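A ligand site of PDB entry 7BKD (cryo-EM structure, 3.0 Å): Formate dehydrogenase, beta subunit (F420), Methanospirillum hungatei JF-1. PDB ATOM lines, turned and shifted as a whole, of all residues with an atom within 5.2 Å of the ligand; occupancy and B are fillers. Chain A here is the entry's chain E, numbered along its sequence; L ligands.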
ATOM      1  N   GLY A  21      21.004  -7.505  -5.688  1.00  0.00           N
ATOM      2  CA  GLY A  21      22.067  -6.532  -5.514  1.00  0.00           C
ATOM      3  C   GLY A  21      23.396  -7.188  -5.247  1.00  0.00           C
ATOM      4  O   GLY A  21      23.473  -8.287  -4.690  1.00  0.00           O
ATOM      5  N   GLU A  22      24.470  -6.512  -5.670  1.00  0.00           N
ATOM      6  CA  GLU A  22      25.801  -7.102  -5.581  1.00  0.00           C
ATOM      7  C   GLU A  22      26.231  -7.284  -4.129  1.00  0.00           C
ATOM      8  O   GLU A  22      26.688  -8.360  -3.732  1.00  0.00           O
ATOM      9  CB  GLU A  22      26.805  -6.251  -6.342  1.00  0.00           C
ATOM     10  CG  GLU A  22      28.181  -6.863  -6.433  1.00  0.00           C
ATOM     11  CD  GLU A  22      28.298  -7.865  -7.563  1.00  0.00           C
ATOM     12  OE1 GLU A  22      29.366  -8.494  -7.708  1.00  0.00           O
ATOM     13  OE2 GLU A  22      27.319  -8.024  -8.317  1.00  0.00           O
ATOM     14  N   CYS A  23      26.091  -6.232  -3.322  1.00  0.00           N
ATOM     15  CA  CYS A  23      26.540  -6.255  -1.937  1.00  0.00           C
ATOM     16  C   CYS A  23      25.486  -5.642  -1.034  1.00  0.00           C
ATOM     17  O   CYS A  23      25.774  -4.778  -0.201  1.00  0.00           O
ATOM     18  CB  CYS A  23      27.873  -5.527  -1.782  1.00  0.00           C
ATOM     19  SG  CYS A  23      29.106  -5.904  -3.056  1.00  0.00           S
ATOM     20  N   GLY A  24      24.229  -6.061  -1.197  1.00  0.00           N
ATOM     21  CA  GLY A  24      23.166  -5.594  -0.342  1.00  0.00           C
ATOM     22  C   GLY A  24      22.116  -4.737  -1.011  1.00  0.00           C
ATOM     23  O   GLY A  24      21.155  -4.334  -0.341  1.00  0.00           O
ATOM     24  N   GLY A  25      22.266  -4.421  -2.292  1.00  0.00           N
ATOM     25  CA  GLY A  25      21.226  -3.721  -3.028  1.00  0.00           C
ATOM     26  C   GLY A  25      20.888  -2.347  -2.495  1.00  0.00           C
ATOM     27  O   GLY A  25      19.767  -1.889  -2.676  1.00  0.00           O
ATOM     28  N   ALA A  26      21.838  -1.684  -1.832  1.00  0.00           N
ATOM     29  CA  ALA A  26      21.558  -0.366  -1.295  1.00  0.00           C
ATOM     30  C   ALA A  26      21.540   0.684  -2.390  1.00  0.00           C
ATOM     31  O   ALA A  26      20.739   1.618  -2.344  1.00  0.00           O
ATOM     32  CB  ALA A  26      22.586  -0.002  -0.218  1.00  0.00           C
ATOM     33  N   VAL A  27      22.430   0.557  -3.376  1.00  0.00           N
ATOM     34  CA  VAL A  27      22.445   1.501  -4.494  1.00  0.00           C
ATOM     35  C   VAL A  27      21.143   1.399  -5.274  1.00  0.00           C
ATOM     36  O   VAL A  27      20.528   2.421  -5.608  1.00  0.00           O
ATOM     37  CB  VAL A  27      23.663   1.233  -5.395  1.00  0.00           C
ATOM     38  CG1 VAL A  27      23.541   2.018  -6.679  1.00  0.00           C
ATOM     39  CG2 VAL A  27      24.933   1.589  -4.672  1.00  0.00           C
ATOM     40  N   THR A  28      20.713   0.182  -5.575  1.00  0.00           N
ATOM     41  CA  THR A  28      19.488  -0.007  -6.346  1.00  0.00           C
ATOM     42  C   THR A  28      18.274   0.451  -5.547  1.00  0.00           C
ATOM     43  O   THR A  28      17.364   1.066  -6.104  1.00  0.00           O
ATOM     44  CB  THR A  28      19.343  -1.463  -6.760  1.00  0.00           C
ATOM     45  OG1 THR A  28      20.379  -1.786  -7.698  1.00  0.00           O
ATOM     46  CG2 THR A  28      17.998  -1.710  -7.408  1.00  0.00           C
ATOM     47  N   LEU A  31      18.255   4.253  -5.708  1.00  0.00           N
ATOM     48  CA  LEU A  31      17.810   4.753  -7.003  1.00  0.00           C
ATOM     49  C   LEU A  31      16.310   4.571  -7.172  1.00  0.00           C
ATOM     50  O   LEU A  31      15.609   5.491  -7.626  1.00  0.00           O
ATOM     51  CB  LEU A  31      18.559   4.042  -8.125  1.00  0.00           C
ATOM     52  CG  LEU A  31      20.035   4.424  -8.275  1.00  0.00           C
ATOM     53  CD1 LEU A  31      20.653   3.706  -9.445  1.00  0.00           C
ATOM     54  CD2 LEU A  31      20.158   5.918  -8.446  1.00  0.00           C
ATOM     55  N   ALA A  45      21.538   4.195 -15.519  1.00  0.00           N
ATOM     56  CA  ALA A  45      22.249   3.084 -14.895  1.00  0.00           C
ATOM     57  C   ALA A  45      22.815   2.152 -15.952  1.00  0.00           C
ATOM     58  O   ALA A  45      22.778   2.455 -17.149  1.00  0.00           O
ATOM     59  CB  ALA A  45      21.333   2.323 -13.952  1.00  0.00           C
ATOM     60  N   ILE A  46      23.331   1.001 -15.528  1.00  0.00           N
ATOM     61  CA  ILE A  46      23.931   0.016 -16.421  1.00  0.00           C
ATOM     62  C   ILE A  46      23.173  -1.289 -16.243  1.00  0.00           C
ATOM     63  O   ILE A  46      22.893  -1.685 -15.105  1.00  0.00           O
ATOM     64  CB  ILE A  46      25.424  -0.169 -16.141  1.00  0.00           C
ATOM     65  CG1 ILE A  46      26.150   1.166 -16.272  1.00  0.00           C
ATOM     66  CG2 ILE A  46      26.018  -1.164 -17.099  1.00  0.00           C
ATOM     67  CD1 ILE A  46      26.082   1.740 -17.633  1.00  0.00           C
ATOM     68  N   LYS A  47      22.832  -1.946 -17.341  1.00  0.00           N
ATOM     69  CA  LYS A  47      22.162  -3.224 -17.277  1.00  0.00           C
ATOM     70  C   LYS A  47      22.825  -4.208 -18.227  1.00  0.00           C
ATOM     71  O   LYS A  47      23.559  -3.826 -19.150  1.00  0.00           O
ATOM     72  CB  LYS A  47      20.668  -3.100 -17.596  1.00  0.00           C
ATOM     73  CG  LYS A  47      20.362  -2.593 -18.986  1.00  0.00           C
ATOM     74  CD  LYS A  47      18.980  -3.033 -19.422  1.00  0.00           C
ATOM     75  CE  LYS A  47      18.708  -2.620 -20.861  1.00  0.00           C
ATOM     76  NZ  LYS A  47      19.646  -3.279 -21.818  1.00  0.00           N
ATOM     77  N   THR A  69      18.637  -3.508 -13.193  1.00  0.00           N
ATOM     78  CA  THR A  69      19.963  -2.915 -13.112  1.00  0.00           C
ATOM     79  C   THR A  69      20.710  -3.302 -11.849  1.00  0.00           C
ATOM     80  O   THR A  69      21.819  -2.801 -11.632  1.00  0.00           O
ATOM     81  CB  THR A  69      19.857  -1.400 -13.195  1.00  0.00           C
ATOM     82  OG1 THR A  69      18.874  -0.945 -12.265  1.00  0.00           O
ATOM     83  CG2 THR A  69      19.477  -0.970 -14.589  1.00  0.00           C
ATOM     84  N   ALA A  70      20.143  -4.154 -11.005  1.00  0.00           N
ATOM     85  CA  ALA A  70      20.826  -4.560  -9.783  1.00  0.00           C
ATOM     86  C   ALA A  70      22.053  -5.395 -10.111  1.00  0.00           C
ATOM     87  O   ALA A  70      22.066  -6.183 -11.051  1.00  0.00           O
ATOM     88  CB  ALA A  70      19.877  -5.354  -8.884  1.00  0.00           C
ATOM     89  N   GLY A  71      23.102  -5.204  -9.318  1.00  0.00           N
ATOM     90  CA  GLY A  71      24.326  -5.948  -9.543  1.00  0.00           C
ATOM     91  C   GLY A  71      25.303  -5.209 -10.424  1.00  0.00           C
ATOM     92  O   GLY A  71      24.931  -4.471 -11.330  1.00  0.00           O
ATOM     93  N   SER A  72      26.584  -5.407 -10.159  1.00  0.00           N
ATOM     94  CA  SER A  72      27.640  -4.734 -10.879  1.00  0.00           C
ATOM     95  C   SER A  72      28.157  -5.613 -12.017  1.00  0.00           C
ATOM     96  O   SER A  72      28.037  -6.833 -12.000  1.00  0.00           O
ATOM     97  CB  SER A  72      28.794  -4.376  -9.957  1.00  0.00           C
ATOM     98  OG  SER A  72      29.692  -5.452  -9.833  1.00  0.00           O
ATOM     99  N   LEU A  73      28.748  -4.949 -13.014  1.00  0.00           N
ATOM    100  CA  LEU A  73      29.329  -5.625 -14.170  1.00  0.00           C
ATOM    101  C   LEU A  73      30.774  -5.153 -14.288  1.00  0.00           C
ATOM    102  O   LEU A  73      31.029  -4.021 -14.702  1.00  0.00           O
ATOM    103  CB  LEU A  73      28.558  -5.316 -15.441  1.00  0.00           C
ATOM    104  CG  LEU A  73      27.062  -5.604 -15.378  1.00  0.00           C
ATOM    105  CD1 LEU A  73      26.380  -5.093 -16.621  1.00  0.00           C
ATOM    106  CD2 LEU A  73      26.822  -7.087 -15.209  1.00  0.00           C
ATOM    107  N   HIS A  74      31.709  -6.023 -13.939  1.00  0.00           N
ATOM    108  CA  HIS A  74      33.117  -5.653 -13.976  1.00  0.00           C
ATOM    109  C   HIS A  74      33.653  -5.560 -15.389  1.00  0.00           C
ATOM    110  O   HIS A  74      34.807  -5.169 -15.559  1.00  0.00           O
ATOM    111  CB  HIS A  74      33.938  -6.632 -13.153  1.00  0.00           C
ATOM    112  CG  HIS A  74      33.677  -6.542 -11.680  1.00  0.00           C
ATOM    113  ND1 HIS A  74      32.432  -6.744 -11.132  1.00  0.00           N
ATOM    114  CD2 HIS A  74      34.499  -6.255 -10.650  1.00  0.00           C
ATOM    115  CE1 HIS A  74      32.495  -6.584  -9.827  1.00  0.00           C
ATOM    116  NE2 HIS A  74      33.746  -6.289  -9.507  1.00  0.00           N
ATOM    117  N   GLY A  76      32.023  -3.673 -17.629  1.00  0.00           N
ATOM    118  CA  GLY A  76      31.519  -2.441 -18.211  1.00  0.00           C
ATOM    119  C   GLY A  76      32.534  -1.328 -18.116  1.00  0.00           C
ATOM    120  O   GLY A  76      32.611  -0.608 -17.121  1.00  0.00           O
ATOM    121  N   THR A  77      33.303  -1.163 -19.194  1.00  0.00           N
ATOM    122  CA  THR A  77      34.345  -0.143 -19.276  1.00  0.00           C
ATOM    123  C   THR A  77      33.862   1.033 -20.106  1.00  0.00           C
ATOM    124  O   THR A  77      34.393   1.334 -21.175  1.00  0.00           O
ATOM    125  CB  THR A  77      35.608  -0.746 -19.863  1.00  0.00           C
ATOM    126  OG1 THR A  77      35.491  -0.796 -21.288  1.00  0.00           O
ATOM    127  CG2 THR A  77      35.820  -2.140 -19.349  1.00  0.00           C
ATOM    128  N   LEU A  78      32.834   1.714 -19.607  1.00  0.00           N
ATOM    129  CA  LEU A  78      32.223   2.808 -20.338  1.00  0.00           C
ATOM    130  C   LEU A  78      31.943   3.958 -19.373  1.00  0.00           C
ATOM    131  O   LEU A  78      31.896   3.773 -18.158  1.00  0.00           O
ATOM    132  CB  LEU A  78      30.953   2.351 -21.053  1.00  0.00           C
ATOM    133  CG  LEU A  78      29.846   1.670 -20.248  1.00  0.00           C
ATOM    134  CD1 LEU A  78      28.852   2.689 -19.741  1.00  0.00           C
ATOM    135  CD2 LEU A  78      29.146   0.636 -21.099  1.00  0.00           C
ATOM    136  N   THR A  99      24.289   6.433 -11.343  1.00  0.00           N
ATOM    137  CA  THR A  99      25.291   5.637 -10.661  1.00  0.00           C
ATOM    138  C   THR A  99      26.582   5.670 -11.459  1.00  0.00           C
ATOM    139  O   THR A  99      26.582   5.559 -12.689  1.00  0.00           O
ATOM    140  CB  THR A  99      24.801   4.209 -10.447  1.00  0.00           C
ATOM    141  OG1 THR A  99      25.738   3.500  -9.621  1.00  0.00           O
ATOM    142  CG2 THR A  99      24.608   3.486 -11.759  1.00  0.00           C
ATOM    143  N   CYS A 100      27.701   5.858 -10.770  1.00  0.00           N
ATOM    144  CA  CYS A 100      28.930   6.213 -11.449  1.00  0.00           C
ATOM    145  C   CYS A 100      30.124   5.607 -10.738  1.00  0.00           C
ATOM    146  O   CYS A 100      30.058   5.276  -9.550  1.00  0.00           O
ATOM    147  CB  CYS A 100      29.063   7.739 -11.554  1.00  0.00           C
ATOM    148  SG  CYS A 100      29.229   8.601  -9.986  1.00  0.00           S
ATOM    149  N   LYS A 101      31.208   5.435 -11.473  1.00  0.00           N
ATOM    150  CA  LYS A 101      32.463   4.996 -10.892  1.00  0.00           C
ATOM    151  C   LYS A 101      33.294   6.214 -10.503  1.00  0.00           C
ATOM    152  O   LYS A 101      32.817   7.355 -10.557  1.00  0.00           O
ATOM    153  CB  LYS A 101      33.216   4.107 -11.878  1.00  0.00           C
ATOM    154  CG  LYS A 101      32.582   2.758 -12.103  1.00  0.00           C
ATOM    155  CD  LYS A 101      33.217   2.065 -13.271  1.00  0.00           C
ATOM    156  CE  LYS A 101      32.797   2.692 -14.577  1.00  0.00           C
ATOM    157  NZ  LYS A 101      33.353   1.943 -15.724  1.00  0.00           N
ATOM    158  N   ASP A 104      33.902   8.050 -13.674  1.00  0.00           N
ATOM    159  CA  ASP A 104      32.659   8.706 -14.074  1.00  0.00           C
ATOM    160  C   ASP A 104      32.437   9.986 -13.284  1.00  0.00           C
ATOM    161  O   ASP A 104      32.014  10.999 -13.846  1.00  0.00           O
ATOM    162  CB  ASP A 104      31.482   7.755 -13.897  1.00  0.00           C
ATOM    163  CG  ASP A 104      31.570   6.544 -14.797  1.00  0.00           C
ATOM    164  OD1 ASP A 104      32.512   6.454 -15.592  1.00  0.00           O
ATOM    165  OD2 ASP A 104      30.678   5.670 -14.712  1.00  0.00           O
ATOM    166  N   VAL A 127      30.324   4.438  -6.871  1.00  0.00           N
ATOM    167  CA  VAL A 127      30.732   3.176  -6.290  1.00  0.00           C
ATOM    168  C   VAL A 127      32.252   3.091  -6.326  1.00  0.00           C
ATOM    169  O   VAL A 127      32.903   3.720  -7.167  1.00  0.00           O
ATOM    170  CB  VAL A 127      30.102   1.971  -7.020  1.00  0.00           C
ATOM    171  CG1 VAL A 127      28.589   2.055  -6.977  1.00  0.00           C
ATOM    172  CG2 VAL A 127      30.585   1.910  -8.456  1.00  0.00           C
ATOM    173  N   ASN A 128      32.818   2.337  -5.393  1.00  0.00           N
ATOM    174  CA  ASN A 128      34.246   2.068  -5.451  1.00  0.00           C
ATOM    175  C   ASN A 128      34.550   1.239  -6.687  1.00  0.00           C
ATOM    176  O   ASN A 128      33.677   0.558  -7.232  1.00  0.00           O
ATOM    177  CB  ASN A 128      34.723   1.343  -4.201  1.00  0.00           C
ATOM    178  CG  ASN A 128      34.248   1.995  -2.928  1.00  0.00           C
ATOM    179  OD1 ASN A 128      33.945   3.177  -2.913  1.00  0.00           O
ATOM    180  ND2 ASN A 128      34.211   1.224  -1.851  1.00  0.00           N
ATOM    181  N   CYS A 129      35.784   1.312  -7.155  1.00  0.00           N
ATOM    182  CA  CYS A 129      36.184   0.569  -8.338  1.00  0.00           C
ATOM    183  C   CYS A 129      37.595   0.043  -8.146  1.00  0.00           C
ATOM    184  O   CYS A 129      38.549   0.812  -8.063  1.00  0.00           O
ATOM    185  CB  CYS A 129      36.091   1.424  -9.594  1.00  0.00           C
ATOM    186  SG  CYS A 129      36.129   0.481 -11.129  1.00  0.00           S
ATOM    187  N   GLY A 130      37.723  -1.281  -8.072  1.00  0.00           N
ATOM    188  CA  GLY A 130      39.024  -1.900  -8.125  1.00  0.00           C
ATOM    189  C   GLY A 130      39.570  -2.088  -9.507  1.00  0.00           C
ATOM    190  O   GLY A 130      40.732  -2.479  -9.662  1.00  0.00           O
ATOM    191  N   GLY A 131      38.771  -1.821 -10.530  1.00  0.00           N
ATOM    192  CA  GLY A 131      39.197  -1.925 -11.909  1.00  0.00           C
ATOM    193  C   GLY A 131      38.167  -2.649 -12.744  1.00  0.00           C
ATOM    194  O   GLY A 131      37.346  -3.420 -12.253  1.00  0.00           O
ATOM    195  N   SER A 132      38.206  -2.390 -14.044  1.00  0.00           N
ATOM    196  CA  SER A 132      37.321  -3.028 -15.005  1.00  0.00           C
ATOM    197  C   SER A 132      38.147  -3.826 -15.998  1.00  0.00           C
ATOM    198  O   SER A 132      39.363  -3.652 -16.103  1.00  0.00           O
ATOM    199  CB  SER A 132      36.464  -2.010 -15.747  1.00  0.00           C
ATOM    200  OG  SER A 132      35.589  -1.336 -14.857  1.00  0.00           O
ATOM    201  N   ILE A 158      35.905  -9.322  -8.997  1.00  0.00           N
ATOM    202  CA  ILE A 158      37.257  -9.126  -8.474  1.00  0.00           C
ATOM    203  C   ILE A 158      37.146  -8.849  -6.990  1.00  0.00           C
ATOM    204  O   ILE A 158      36.687  -7.776  -6.585  1.00  0.00           O
ATOM    205  CB  ILE A 158      37.994  -7.977  -9.181  1.00  0.00           C
ATOM    206  CG1 ILE A 158      38.106  -8.249 -10.679  1.00  0.00           C
ATOM    207  CG2 ILE A 158      39.356  -7.768  -8.570  1.00  0.00           C
ATOM    208  CD1 ILE A 158      38.492  -7.031 -11.492  1.00  0.00           C
ATOM    209  N   ALA A 205      29.454   4.128  -2.364  1.00  0.00           N
ATOM    210  CA  ALA A 205      29.004   2.806  -1.948  1.00  0.00           C
ATOM    211  C   ALA A 205      30.001   1.741  -2.359  1.00  0.00           C
ATOM    212  O   ALA A 205      30.487   1.735  -3.502  1.00  0.00           O
ATOM    213  CB  ALA A 205      27.642   2.497  -2.552  1.00  0.00           C
ATOM    214  N   GLY A 206      30.304   0.833  -1.438  1.00  0.00           N
ATOM    215  CA  GLY A 206      31.213  -0.245  -1.745  1.00  0.00           C
ATOM    216  C   GLY A 206      30.959  -1.443  -0.857  1.00  0.00           C
ATOM    217  O   GLY A 206      29.958  -1.516  -0.149  1.00  0.00           O
ATOM    218  N   ASN A 207      31.900  -2.391  -0.909  1.00  0.00           N
ATOM    219  CA  ASN A 207      31.861  -3.540  -0.013  1.00  0.00           C
ATOM    220  C   ASN A 207      33.142  -3.698   0.789  1.00  0.00           C
ATOM    221  O   ASN A 207      33.325  -4.721   1.456  1.00  0.00           O
ATOM    222  CB  ASN A 207      31.552  -4.825  -0.803  1.00  0.00           C
ATOM    223  CG  ASN A 207      32.653  -5.220  -1.773  1.00  0.00           C
ATOM    224  OD1 ASN A 207      33.831  -4.991  -1.549  1.00  0.00           O
ATOM    225  ND2 ASN A 207      32.238  -5.810  -2.887  1.00  0.00           N
ATOM    226  N   TRP A 208      34.044  -2.723   0.727  1.00  0.00           N
ATOM    227  CA  TRP A 208      35.189  -2.717   1.629  1.00  0.00           C
ATOM    228  C   TRP A 208      34.746  -2.261   3.012  1.00  0.00           C
ATOM    229  O   TRP A 208      33.937  -1.338   3.145  1.00  0.00           O
ATOM    230  CB  TRP A 208      36.278  -1.786   1.107  1.00  0.00           C
ATOM    231  CG  TRP A 208      36.974  -2.279  -0.102  1.00  0.00           C
ATOM    232  CD1 TRP A 208      37.063  -3.556  -0.528  1.00  0.00           C
ATOM    233  CD2 TRP A 208      37.694  -1.498  -1.056  1.00  0.00           C
ATOM    234  NE1 TRP A 208      37.790  -3.630  -1.683  1.00  0.00           N
ATOM    235  CE2 TRP A 208      38.192  -2.376  -2.028  1.00  0.00           C
ATOM    236  CE3 TRP A 208      37.961  -0.135  -1.178  1.00  0.00           C
ATOM    237  CZ2 TRP A 208      38.947  -1.932  -3.108  1.00  0.00           C
ATOM    238  CZ3 TRP A 208      38.709   0.306  -2.251  1.00  0.00           C
ATOM    239  CH2 TRP A 208      39.187  -0.597  -3.196  1.00  0.00           C
ATOM    240  N   THR A 219      26.061  -3.061   2.431  1.00  0.00           N
ATOM    241  CA  THR A 219      26.842  -2.150   1.598  1.00  0.00           C
ATOM    242  C   THR A 219      27.405  -1.050   2.490  1.00  0.00           C
ATOM    243  O   THR A 219      26.696  -0.483   3.318  1.00  0.00           O
ATOM    244  CB  THR A 219      25.984  -1.529   0.494  1.00  0.00           C
ATOM    245  OG1 THR A 219      25.377  -2.578  -0.267  1.00  0.00           O
ATOM    246  CG2 THR A 219      26.826  -0.684  -0.422  1.00  0.00           C
ATOM    247  N   MET A 261      45.748  -0.162  -2.493  1.00  0.00           N
ATOM    248  CA  MET A 261      45.406   0.111  -3.883  1.00  0.00           C
ATOM    249  C   MET A 261      46.159   1.318  -4.417  1.00  0.00           C
ATOM    250  O   MET A 261      46.602   1.320  -5.574  1.00  0.00           O
ATOM    251  CB  MET A 261      43.898   0.324  -4.010  1.00  0.00           C
ATOM    252  CG  MET A 261      43.118  -0.942  -4.332  1.00  0.00           C
ATOM    253  SD  MET A 261      43.353  -1.448  -6.040  1.00  0.00           S
ATOM    254  CE  MET A 261      42.034  -2.627  -6.229  1.00  0.00           C
HETATM  255  P1  LIG L   1      23.874  -2.654  -6.550  1.00  0.00           P
HETATM  256  O1  LIG L   1      24.613  -3.841  -6.998  1.00  0.00           O
HETATM  257  O2  LIG L   1      22.440  -2.864  -6.107  1.00  0.00           O
HETATM  258  O3  LIG L   1      23.916  -1.574  -7.638  1.00  0.00           O
HETATM  259  C1  LIG L   1      25.011  -1.489  -8.563  1.00  0.00           C
HETATM  260  C2  LIG L   1      24.820  -0.266  -9.428  1.00  0.00           C
HETATM  261  O4  LIG L   1      25.996  -0.051 -10.224  1.00  0.00           O
HETATM  262  C3  LIG L   1      23.641  -0.332 -10.392  1.00  0.00           C
HETATM  263  O5  LIG L   1      22.950   0.901 -10.454  1.00  0.00           O
HETATM  264  C4  LIG L   1      24.317  -0.653 -11.727  1.00  0.00           C
HETATM  265  O6  LIG L   1      23.577  -0.112 -12.817  1.00  0.00           O
HETATM  266  C5  LIG L   1      25.642   0.087 -11.575  1.00  0.00           C
HETATM  267  N1  LIG L   1      26.725  -0.444 -12.393  1.00  0.00           N
HETATM  268  C6  LIG L   1      26.956  -1.751 -12.693  1.00  0.00           C
HETATM  269  N2  LIG L   1      28.009  -1.944 -13.446  1.00  0.00           N
HETATM  270  C7  LIG L   1      28.501  -0.665 -13.663  1.00  0.00           C
HETATM  271  C8  LIG L   1      29.600  -0.176 -14.390  1.00  0.00           C
HETATM  272  N3  LIG L   1      30.453  -0.956 -15.064  1.00  0.00           N
HETATM  273  N4  LIG L   1      29.802   1.152 -14.392  1.00  0.00           N
HETATM  274  C9  LIG L   1      28.961   1.942 -13.713  1.00  0.00           C
HETATM  275  N5  LIG L   1      27.893   1.594 -13.000  1.00  0.00           N
HETATM  276  C10 LIG L   1      27.714   0.268 -13.018  1.00  0.00           C
HETATM  277  N6  LIG L   1      33.475  -2.357  -4.772  1.00  0.00           N
HETATM  278  C11 LIG L   1      34.479  -2.714  -3.924  1.00  0.00           C
HETATM  279  O7  LIG L   1      34.345  -2.658  -2.706  1.00  0.00           O
HETATM  280  N7  LIG L   1      35.681  -3.146  -4.448  1.00  0.00           N
HETATM  281  C12 LIG L   1      35.989  -3.269  -5.780  1.00  0.00           C
HETATM  282  O8  LIG L   1      37.096  -3.674  -6.133  1.00  0.00           O
HETATM  283  C13 LIG L   1      34.914  -2.888  -6.669  1.00  0.00           C
HETATM  284  N8  LIG L   1      35.108  -2.966  -7.944  1.00  0.00           N
HETATM  285  C14 LIG L   1      34.081  -2.604  -8.785  1.00  0.00           C
HETATM  286  C15 LIG L   1      34.278  -2.678 -10.157  1.00  0.00           C
HETATM  287  C16 LIG L   1      33.270  -2.318 -11.042  1.00  0.00           C
HETATM  288  C17 LIG L   1      33.512  -2.418 -12.528  1.00  0.00           C
HETATM  289  C18 LIG L   1      32.026  -1.873 -10.545  1.00  0.00           C
HETATM  290  C19 LIG L   1      30.918  -1.485 -11.471  1.00  0.00           C
HETATM  291  C20 LIG L   1      31.829  -1.799  -9.173  1.00  0.00           C
HETATM  292  C21 LIG L   1      32.844  -2.156  -8.294  1.00  0.00           C
HETATM  293  N9  LIG L   1      32.669  -2.095  -6.902  1.00  0.00           N
HETATM  294  C22 LIG L   1      33.680  -2.449  -6.060  1.00  0.00           C
HETATM  295  C23 LIG L   1      31.407  -1.642  -6.320  1.00  0.00           C
HETATM  296  C24 LIG L   1      30.550  -2.781  -5.789  1.00  0.00           C
HETATM  297  O9  LIG L   1      29.850  -3.419  -6.861  1.00  0.00           O
HETATM  298  C25 LIG L   1      29.544  -2.226  -4.791  1.00  0.00           C
HETATM  299  O10 LIG L   1      29.698  -2.900  -3.555  1.00  0.00           O
HETATM  300  C26 LIG L   1      28.099  -2.377  -5.249  1.00  0.00           C
HETATM  301  O11 LIG L   1      28.056  -2.254  -6.666  1.00  0.00           O
HETATM  302  C27 LIG L   1      27.185  -1.378  -4.586  1.00  0.00           C
HETATM  303  O12 LIG L   1      26.368  -2.058  -3.606  1.00  0.00           O
HETATM  304  P2  LIG L   1      24.955  -2.627  -3.971  1.00  0.00           P
HETATM  305  O13 LIG L   1      25.023  -4.141  -4.207  1.00  0.00           O
HETATM  306  O14 LIG L   1      23.988  -2.178  -2.989  1.00  0.00           O
HETATM  307  O15 LIG L   1      24.651  -1.948  -5.357  1.00  0.00           O
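The backbone NH of Ala 26 is in hydrogen-bond range of an oxygen (O14) of the ligand (2.5 Å). O13 of the ligand lies within hydrogen-bond range of N of Cys 23, 2.5 Å away. The side-chain sulfur of Cys 23 is in hydrogen-bond range of an oxygen (O10) of the ligand (3.1 Å). The backbone NH (N) of Asn 207 lies within hydrogen-bond range of an oxygen (O7) of the ligand (3.0 Å). O7 of the ligand sits close to OD1 of Asn 207. O2 of the ligand is in hydrogen-bond range of OG1 of Thr 28. An oxygen (O13) of the ligand sits at hydrogen-bond distance from the backbone NH of Glu 22 (2.8 Å). N of Ile 46 sits at hydrogen-bond distance from O6 of the ligand. The backbone carbonyl oxygen (O) of Ile 46 sits at hydrogen-bond distance from an oxygen (O6) of the ligand, at 2.9 Å. An oxygen (O14) of the ligand sits at hydrogen-bond distance from the backbone NH (N) of Gly 25 (2.9 Å). O of Gly 76 sits at hydrogen-bond distance from N3 of the ligand (3.0 Å). An oxygen (O14) of the ligand is in hydrogen-bond range of the side-chain hydroxyl of Thr 219 (3.1 Å). The backbone NH (N) of Gly 71 sits at hydrogen-bond distance from an oxygen (O1) of the ligand, 3.1 Å away. The backbone NH of Gly 130 lies within hydrogen-bond range of a nitrogen (N8) of the ligand (3.1 Å). N2 of the ligand is in hydrogen-bond range of N of Leu 73, 3.1 Å away. The backbone carbonyl oxygen of Leu 73 lies within hydrogen-bond range of a nitrogen (N3) of the ligand (3.1 Å). N of Val 27 sits at hydrogen-bond distance from O14 of the ligand (3.2 Å). The backbone carbonyl oxygen of Thr 69 sits close to an oxygen (O6) of the ligand. The backbone NH (N) of Trp 208 sits at hydrogen-bond distance from an oxygen (O7) of the ligand, at 3.4 Å.
The side-chain sulfur (SG) of Cys 23 is in hydrogen-bond range of the side-chain amide nitrogen (ND2) of Asn 207 (3.1 Å). The backbone carbonyl oxygen (O) of Cys 23 lies within hydrogen-bond range of the backbone NH (N) of Thr 219, at 3.2 Å. The side-chain carboxylate of Glu 22 is in hydrogen-bond range of the backbone NH of Ser 72, at 3.3 Å. O of Ala 205 sits at hydrogen-bond distance from N of Asn 128, at 3.1 Å. The backbone carbonyl oxygen (O) of Gly 76 lies within hydrogen-bond range of the side-chain amino group (NZ) of Lys 101 (3.0 Å). The backbone carbonyl oxygen (O) of Leu 78 is in hydrogen-bond range of the side-chain amino group (NZ) of Lys 101. A ring nitrogen (ND1) of His 74 lies close to the side-chain hydroxyl (OG) of Ser 72 (3.3 Å). N of Val 127 lies within hydrogen-bond range of O of Cys 100 (2.8 Å).
N9 of the ligand sits close to O of Asn 128, at 2.9 Å. C of Gly 21 touches O13 of the ligand, at 3.6 Å. N of Gly 24 touches O13 of the ligand (3.7 Å). CD1 of Leu 31 touches O5 of the ligand (3.8 Å). Ala 45 touches the ligand (CB to O6, 3.5 Å). Ser 72 touches the ligand. CA of His 74 touches C17 of the ligand, 3.6 Å away. CG2 of Thr 99 touches O5 of the ligand, at 3.3 Å. Lys 101 touches the ligand (CE to N4, 3.4 Å). Val 127 touches the ligand (CB to C23, 3.9 Å). Cys 129 touches the ligand. Gly 131 touches the ligand (O to C15, 3.8 Å). Ser 132 touches the ligand. Gly 206 touches the ligand. 29 residues have an atom within 4 Å of the ligand: Gly 21, Glu 22, Cys 23, Gly 24, Gly 25, Ala 26, Val 27, Thr 28, Leu 31, Ala 45, Ile 46, Thr 69, Gly 71, Ser 72, Leu 73, His 74, Gly 76, Thr 99, Lys 101, Val 127, Asn 128, Cys 129, Gly 130, Gly 131, Ser 132, Gly 206, Asn 207, Trp 208 and Thr 219. The nearest printed residue that does not touch the ligand is Ile 158 (4.1 Å).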
